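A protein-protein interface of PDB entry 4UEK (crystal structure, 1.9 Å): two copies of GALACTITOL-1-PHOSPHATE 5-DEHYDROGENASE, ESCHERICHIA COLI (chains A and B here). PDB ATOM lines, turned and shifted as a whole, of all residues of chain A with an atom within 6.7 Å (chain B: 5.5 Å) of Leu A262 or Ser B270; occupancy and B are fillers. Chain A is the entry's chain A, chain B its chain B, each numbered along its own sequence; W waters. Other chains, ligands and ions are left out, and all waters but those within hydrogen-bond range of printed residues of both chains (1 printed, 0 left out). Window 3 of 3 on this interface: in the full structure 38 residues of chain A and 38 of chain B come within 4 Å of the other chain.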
ATOM      1  N   LYS A  47      -8.089 -13.853 -29.097  1.00  0.00           N
ATOM      2  CA  LYS A  47      -8.916 -13.286 -28.036  1.00  0.00           C
ATOM      3  C   LYS A  47      -8.106 -12.298 -27.209  1.00  0.00           C
ATOM      4  O   LYS A  47      -8.375 -12.093 -26.025  1.00  0.00           O
ATOM      5  CB  LYS A  47      -9.499 -14.397 -27.161  1.00  0.00           C
ATOM      6  CG  LYS A  47     -10.524 -15.256 -27.893  1.00  0.00           C
ATOM      7  CD  LYS A  47     -10.832 -16.557 -27.161  1.00  0.00           C
ATOM      8  CE  LYS A  47     -11.448 -16.302 -25.786  1.00  0.00           C
ATOM      9  NZ  LYS A  47     -11.756 -17.576 -25.067  1.00  0.00           N
ATOM     10  N   GLU A 235      -9.853 -32.765 -16.954  1.00  0.00           N
ATOM     11  CA  GLU A 235     -10.578 -31.767 -17.731  1.00  0.00           C
ATOM     12  C   GLU A 235      -9.554 -31.015 -18.571  1.00  0.00           C
ATOM     13  O   GLU A 235      -8.813 -30.180 -18.043  1.00  0.00           O
ATOM     14  CB  GLU A 235     -11.345 -30.806 -16.812  1.00  0.00           C
ATOM     15  CG  GLU A 235     -12.434 -29.986 -17.506  1.00  0.00           C
ATOM     16  CD  GLU A 235     -11.945 -29.212 -18.724  1.00  0.00           C
ATOM     17  OE1 GLU A 235     -11.086 -28.305 -18.579  1.00  0.00           O
ATOM     18  OE2 GLU A 235     -12.399 -29.550 -19.837  1.00  0.00           O
ATOM     19  N   ALA A 237     -10.429 -29.640 -21.856  1.00  0.00           N
ATOM     20  CA  ALA A 237     -11.093 -28.770 -22.824  1.00  0.00           C
ATOM     21  C   ALA A 237     -11.006 -27.291 -22.448  1.00  0.00           C
ATOM     22  O   ALA A 237     -10.924 -26.425 -23.319  1.00  0.00           O
ATOM     23  CB  ALA A 237     -12.545 -29.184 -22.990  1.00  0.00           C
ATOM     24  N   GLY A 238     -11.040 -26.996 -21.154  1.00  0.00           N
ATOM     25  CA  GLY A 238     -10.821 -25.634 -20.704  1.00  0.00           C
ATOM     26  C   GLY A 238     -11.964 -24.706 -21.051  1.00  0.00           C
ATOM     27  O   GLY A 238     -11.763 -23.544 -21.407  1.00  0.00           O
ATOM     28  N   VAL A 239     -13.178 -25.220 -20.961  1.00  0.00           N
ATOM     29  CA  VAL A 239     -14.343 -24.384 -21.147  1.00  0.00           C
ATOM     30  C   VAL A 239     -15.266 -24.685 -19.973  1.00  0.00           C
ATOM     31  O   VAL A 239     -15.204 -25.777 -19.398  1.00  0.00           O
ATOM     32  CB  VAL A 239     -15.034 -24.631 -22.509  1.00  0.00           C
ATOM     33  CG1 VAL A 239     -14.141 -24.165 -23.662  1.00  0.00           C
ATOM     34  CG2 VAL A 239     -15.400 -26.087 -22.669  1.00  0.00           C
ATOM     35  N   PRO A 240     -16.108 -23.714 -19.589  1.00  0.00           N
ATOM     36  CA  PRO A 240     -16.871 -23.889 -18.347  1.00  0.00           C
ATOM     37  C   PRO A 240     -17.847 -25.071 -18.385  1.00  0.00           C
ATOM     38  O   PRO A 240     -18.053 -25.712 -17.356  1.00  0.00           O
ATOM     39  CB  PRO A 240     -17.622 -22.560 -18.202  1.00  0.00           C
ATOM     40  CG  PRO A 240     -17.611 -21.941 -19.555  1.00  0.00           C
ATOM     41  CD  PRO A 240     -16.353 -22.406 -20.219  1.00  0.00           C
ATOM     42  N   THR A 242     -17.440 -27.994 -19.663  1.00  0.00           N
ATOM     43  CA  THR A 242     -16.795 -29.276 -19.386  1.00  0.00           C
ATOM     44  C   THR A 242     -16.332 -29.389 -17.943  1.00  0.00           C
ATOM     45  O   THR A 242     -16.209 -30.498 -17.429  1.00  0.00           O
ATOM     46  CB  THR A 242     -15.582 -29.538 -20.304  1.00  0.00           C
ATOM     47  OG1 THR A 242     -14.646 -28.458 -20.175  1.00  0.00           O
ATOM     48  CG2 THR A 242     -16.026 -29.687 -21.761  1.00  0.00           C
ATOM     49  N   VAL A 243     -16.042 -28.265 -17.297  1.00  0.00           N
ATOM     50  CA  VAL A 243     -15.761 -28.315 -15.869  1.00  0.00           C
ATOM     51  C   VAL A 243     -17.036 -28.742 -15.143  1.00  0.00           C
ATOM     52  O   VAL A 243     -17.006 -29.599 -14.246  1.00  0.00           O
ATOM     53  CB  VAL A 243     -15.269 -26.960 -15.301  1.00  0.00           C
ATOM     54  CG1 VAL A 243     -15.147 -27.038 -13.794  1.00  0.00           C
ATOM     55  CG2 VAL A 243     -13.932 -26.582 -15.897  1.00  0.00           C
ATOM     56  N   GLY A 260      -7.158 -27.720 -18.154  1.00  0.00           N
ATOM     57  CA  GLY A 260      -7.587 -26.692 -19.086  1.00  0.00           C
ATOM     58  C   GLY A 260      -7.831 -25.352 -18.424  1.00  0.00           C
ATOM     59  O   GLY A 260      -8.602 -25.242 -17.468  1.00  0.00           O
ATOM     60  N   THR A 261      -7.171 -24.320 -18.937  1.00  0.00           N
ATOM     61  CA  THR A 261      -7.367 -22.973 -18.424  1.00  0.00           C
ATOM     62  C   THR A 261      -8.632 -22.362 -19.022  1.00  0.00           C
ATOM     63  O   THR A 261      -8.866 -22.455 -20.230  1.00  0.00           O
ATOM     64  CB  THR A 261      -6.148 -22.076 -18.735  1.00  0.00           C
ATOM     65  OG1 THR A 261      -5.078 -22.414 -17.845  1.00  0.00           O
ATOM     66  CG2 THR A 261      -6.491 -20.614 -18.556  1.00  0.00           C
ATOM     67  N   LEU A 262      -9.455 -21.746 -18.180  1.00  0.00           N
ATOM     68  CA  LEU A 262     -10.647 -21.070 -18.677  1.00  0.00           C
ATOM     69  C   LEU A 262     -10.331 -19.668 -19.201  1.00  0.00           C
ATOM     70  O   LEU A 262      -9.448 -18.982 -18.692  1.00  0.00           O
ATOM     71  CB  LEU A 262     -11.710 -20.995 -17.587  1.00  0.00           C
ATOM     72  CG  LEU A 262     -12.749 -22.115 -17.541  1.00  0.00           C
ATOM     73  CD1 LEU A 262     -12.124 -23.482 -17.737  1.00  0.00           C
ATOM     74  CD2 LEU A 262     -13.470 -22.045 -16.209  1.00  0.00           C
ATOM     75  N   HIS A 263     -11.053 -19.254 -20.236  1.00  0.00           N
ATOM     76  CA  HIS A 263     -10.948 -17.898 -20.746  1.00  0.00           C
ATOM     77  C   HIS A 263     -12.323 -17.269 -20.677  1.00  0.00           C
ATOM     78  O   HIS A 263     -12.568 -16.182 -21.201  1.00  0.00           O
ATOM     79  CB  HIS A 263     -10.385 -17.891 -22.168  1.00  0.00           C
ATOM     80  CG  HIS A 263      -8.953 -18.319 -22.234  1.00  0.00           C
ATOM     81  ND1 HIS A 263      -7.907 -17.420 -22.262  1.00  0.00           N
ATOM     82  CD2 HIS A 263      -8.390 -19.552 -22.230  1.00  0.00           C
ATOM     83  CE1 HIS A 263      -6.763 -18.081 -22.295  1.00  0.00           C
ATOM     84  NE2 HIS A 263      -7.029 -19.376 -22.277  1.00  0.00           N
ATOM     85  N   GLN A 264     -13.215 -17.979 -19.999  1.00  0.00           N
ATOM     86  CA  GLN A 264     -14.563 -17.510 -19.754  1.00  0.00           C
ATOM     87  C   GLN A 264     -14.884 -17.831 -18.303  1.00  0.00           C
ATOM     88  O   GLN A 264     -14.404 -18.836 -17.784  1.00  0.00           O
ATOM     89  CB  GLN A 264     -15.544 -18.192 -20.705  1.00  0.00           C
ATOM     90  CG  GLN A 264     -16.946 -17.653 -20.654  1.00  0.00           C
ATOM     91  CD  GLN A 264     -17.839 -18.300 -21.692  1.00  0.00           C
ATOM     92  OE1 GLN A 264     -17.378 -19.107 -22.507  1.00  0.00           O
ATOM     93  NE2 GLN A 264     -19.125 -17.959 -21.665  1.00  0.00           N
ATOM     94  N   ASP A 265     -15.668 -16.978 -17.642  1.00  0.00           N
ATOM     95  CA  ASP A 265     -16.056 -17.206 -16.245  1.00  0.00           C
ATOM     96  C   ASP A 265     -16.803 -18.531 -16.040  1.00  0.00           C
ATOM     97  O   ASP A 265     -17.428 -19.047 -16.957  1.00  0.00           O
ATOM     98  CB  ASP A 265     -16.912 -16.044 -15.747  1.00  0.00           C
ATOM     99  CG  ASP A 265     -16.104 -14.771 -15.543  1.00  0.00           C
ATOM    100  OD1 ASP A 265     -14.902 -14.766 -15.889  1.00  0.00           O
ATOM    101  OD2 ASP A 265     -16.662 -13.782 -15.024  1.00  0.00           O
ATOM    102  N   LEU A 266     -16.716 -19.081 -14.834  1.00  0.00           N
ATOM    103  CA  LEU A 266     -17.398 -20.326 -14.485  1.00  0.00           C
ATOM    104  C   LEU A 266     -18.573 -20.078 -13.543  1.00  0.00           C
ATOM    105  O   LEU A 266     -18.392 -19.588 -12.425  1.00  0.00           O
ATOM    106  CB  LEU A 266     -16.428 -21.309 -13.826  1.00  0.00           C
ATOM    107  CG  LEU A 266     -17.051 -22.612 -13.331  1.00  0.00           C
ATOM    108  CD1 LEU A 266     -17.488 -23.447 -14.512  1.00  0.00           C
ATOM    109  CD2 LEU A 266     -16.068 -23.376 -12.461  1.00  0.00           C
ATOM    110  N   LEU B 268     -17.448 -17.936 -10.315  1.00  0.00           N
ATOM    111  CA  LEU B 268     -16.029 -17.630 -10.175  1.00  0.00           C
ATOM    112  C   LEU B 268     -15.545 -16.950 -11.443  1.00  0.00           C
ATOM    113  O   LEU B 268     -15.816 -17.422 -12.537  1.00  0.00           O
ATOM    114  CB  LEU B 268     -15.210 -18.893  -9.907  1.00  0.00           C
ATOM    115  CG  LEU B 268     -15.471 -19.675  -8.618  1.00  0.00           C
ATOM    116  CD1 LEU B 268     -14.594 -20.924  -8.574  1.00  0.00           C
ATOM    117  CD2 LEU B 268     -15.224 -18.814  -7.394  1.00  0.00           C
ATOM    118  N   THR B 269     -14.836 -15.837 -11.311  1.00  0.00           N
ATOM    119  CA  THR B 269     -14.239 -15.242 -12.489  1.00  0.00           C
ATOM    120  C   THR B 269     -13.241 -16.210 -13.095  1.00  0.00           C
ATOM    121  O   THR B 269     -12.751 -17.136 -12.429  1.00  0.00           O
ATOM    122  CB  THR B 269     -13.513 -13.921 -12.191  1.00  0.00           C
ATOM    123  OG1 THR B 269     -12.359 -14.189 -11.384  1.00  0.00           O
ATOM    124  CG2 THR B 269     -14.434 -12.941 -11.474  1.00  0.00           C
ATOM    125  N   SER B 270     -12.945 -15.989 -14.366  1.00  0.00           N
ATOM    126  CA  SER B 270     -11.914 -16.732 -15.067  1.00  0.00           C
ATOM    127  C   SER B 270     -10.578 -16.655 -14.327  1.00  0.00           C
ATOM    128  O   SER B 270      -9.857 -17.646 -14.215  1.00  0.00           O
ATOM    129  CB  SER B 270     -11.784 -16.187 -16.495  1.00  0.00           C
ATOM    130  OG  SER B 270     -10.464 -16.313 -16.971  1.00  0.00           O
ATOM    131  N   ALA B 271     -10.259 -15.470 -13.819  1.00  0.00           N
ATOM    132  CA  ALA B 271      -9.048 -15.253 -13.029  1.00  0.00           C
ATOM    133  C   ALA B 271      -9.003 -16.096 -11.758  1.00  0.00           C
ATOM    134  O   ALA B 271      -7.983 -16.727 -11.469  1.00  0.00           O
ATOM    135  CB  ALA B 271      -8.913 -13.779 -12.664  1.00  0.00           C
ATOM    136  N   THR B 272     -10.085 -16.080 -10.980  1.00  0.00           N
ATOM    137  CA  THR B 272     -10.122 -16.855  -9.739  1.00  0.00           C
ATOM    138  C   THR B 272     -10.004 -18.360  -9.997  1.00  0.00           C
ATOM    139  O   THR B 272      -9.242 -19.050  -9.322  1.00  0.00           O
ATOM    140  CB  THR B 272     -11.413 -16.598  -8.927  1.00  0.00           C
ATOM    141  OG1 THR B 272     -11.478 -15.221  -8.537  1.00  0.00           O
ATOM    142  CG2 THR B 272     -11.420 -17.458  -7.682  1.00  0.00           C
ATOM    143  N   PHE B 273     -10.753 -18.870 -10.973  1.00  0.00           N
ATOM    144  CA  PHE B 273     -10.656 -20.282 -11.330  1.00  0.00           C
ATOM    145  C   PHE B 273      -9.217 -20.625 -11.687  1.00  0.00           C
ATOM    146  O   PHE B 273      -8.698 -21.667 -11.297  1.00  0.00           O
ATOM    147  CB  PHE B 273     -11.580 -20.611 -12.513  1.00  0.00           C
ATOM    148  CG  PHE B 273     -11.454 -22.030 -13.003  1.00  0.00           C
ATOM    149  CD1 PHE B 273     -12.186 -23.043 -12.417  1.00  0.00           C
ATOM    150  CD2 PHE B 273     -10.605 -22.346 -14.050  1.00  0.00           C
ATOM    151  CE1 PHE B 273     -12.075 -24.360 -12.863  1.00  0.00           C
ATOM    152  CE2 PHE B 273     -10.491 -23.652 -14.505  1.00  0.00           C
ATOM    153  CZ  PHE B 273     -11.228 -24.661 -13.904  1.00  0.00           C
ATOM    154  N   GLY B 274      -8.594 -19.734 -12.450  1.00  0.00           N
ATOM    155  CA  GLY B 274      -7.228 -19.907 -12.905  1.00  0.00           C
ATOM    156  C   GLY B 274      -6.258 -20.071 -11.756  1.00  0.00           C
ATOM    157  O   GLY B 274      -5.260 -20.769 -11.891  1.00  0.00           O
ATOM    158  N   LYS B 275      -6.555 -19.435 -10.621  1.00  0.00           N
ATOM    159  CA  LYS B 275      -5.691 -19.539  -9.442  1.00  0.00           C
ATOM    160  C   LYS B 275      -5.720 -20.938  -8.842  1.00  0.00           C
ATOM    161  O   LYS B 275      -4.737 -21.382  -8.233  1.00  0.00           O
ATOM    162  CB  LYS B 275      -6.090 -18.507  -8.386  1.00  0.00           C
ATOM    163  CG  LYS B 275      -5.774 -17.069  -8.797  1.00  0.00           C
ATOM    164  CD  LYS B 275      -6.237 -16.092  -7.710  1.00  0.00           C
ATOM    165  CE  LYS B 275      -5.903 -14.651  -8.052  1.00  0.00           C
ATOM    166  NZ  LYS B 275      -4.449 -14.372  -7.944  1.00  0.00           N
HETATM  167  O   HOH W   1      -8.820 -19.628 -16.027  1.00  0.00           O
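The side-chain carboxylate of Asp A265 sits at hydrogen-bond distance from the backbone NH of Ser B270, 2.8 Å away. The backbone carbonyl oxygen (O) of Leu A262 lies within hydrogen-bond range of the side-chain hydroxyl (OG) of Ser B270. The backbone carbonyl oxygen of Leu A266 lies within hydrogen-bond range of the backbone NH of Leu B268 (2.8 Å).
OG1 of Thr B269 sits at hydrogen-bond distance from N of Thr B272 (3.0 Å). The backbone carbonyl oxygen (O) of Glu A235 sits at hydrogen-bond distance from the backbone NH (N) of Gly A260. The backbone NH (N) of Ala B271 lies close to the side-chain hydroxyl (OG1) of Thr B269, 3.5 Å away.
Val A243 touches Phe B273 (CG2 to CZ, 3.9 Å). Phe B273 touches Gly A260 (CE2 to O, 3.9 Å). Leu A262 touches Phe B273 (CD2 to CD2, 3.6 Å). O of Gln A264 touches CB of Ser B270 (3.9 Å). Leu B268 touches Asp A265. Thr B269 touches Asp A265. Leu A266 touches Phe B273.
Ser B270 touches three residues of chain A. Of the printed residues of chain A, Thr B269 touches Asp A265. Printed residues of chain B within 4 Å of Val A243: Phe B273 (3.9 Å). Of the printed residues of chain A, Phe B273 touches Val A243 (3.9 Å), Gly A260 (3.9 Å), Leu A262 (3.6 Å) and Leu A266 (3.9 Å). Lys B275 touches none of the printed residues of chain A.
Of the 8 printed residues of chain B, 4 touch a printed residue of chain A. Printed residues of chain B that touch a printed residue of chain A: Leu B268, Thr B269, Ser B270 and Phe B273. Hydrophobic or aromatic side chains of chain B within 4 Å of the printed part of chain A: Phe B273. Of the 15 printed residues of chain A, 6 touch a printed residue of chain B. Printed residues of chain A that touch a printed residue of chain B: Val A243, Gly A260, Leu A262, Gln A264, Asp A265 and Leu A266. Among the printed residues, 10 pairs touch across the chains. Among the printed residues, no Asp or Glu carboxylate lies within 4 Å of a Lys or Arg side-chain nitrogen of the other chain.
No position is printed for both chains.
Water W1 bridges the backbone carbonyl oxygen (O) of Leu A262 and the backbone carbonyl oxygen (O) of Ser B270.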
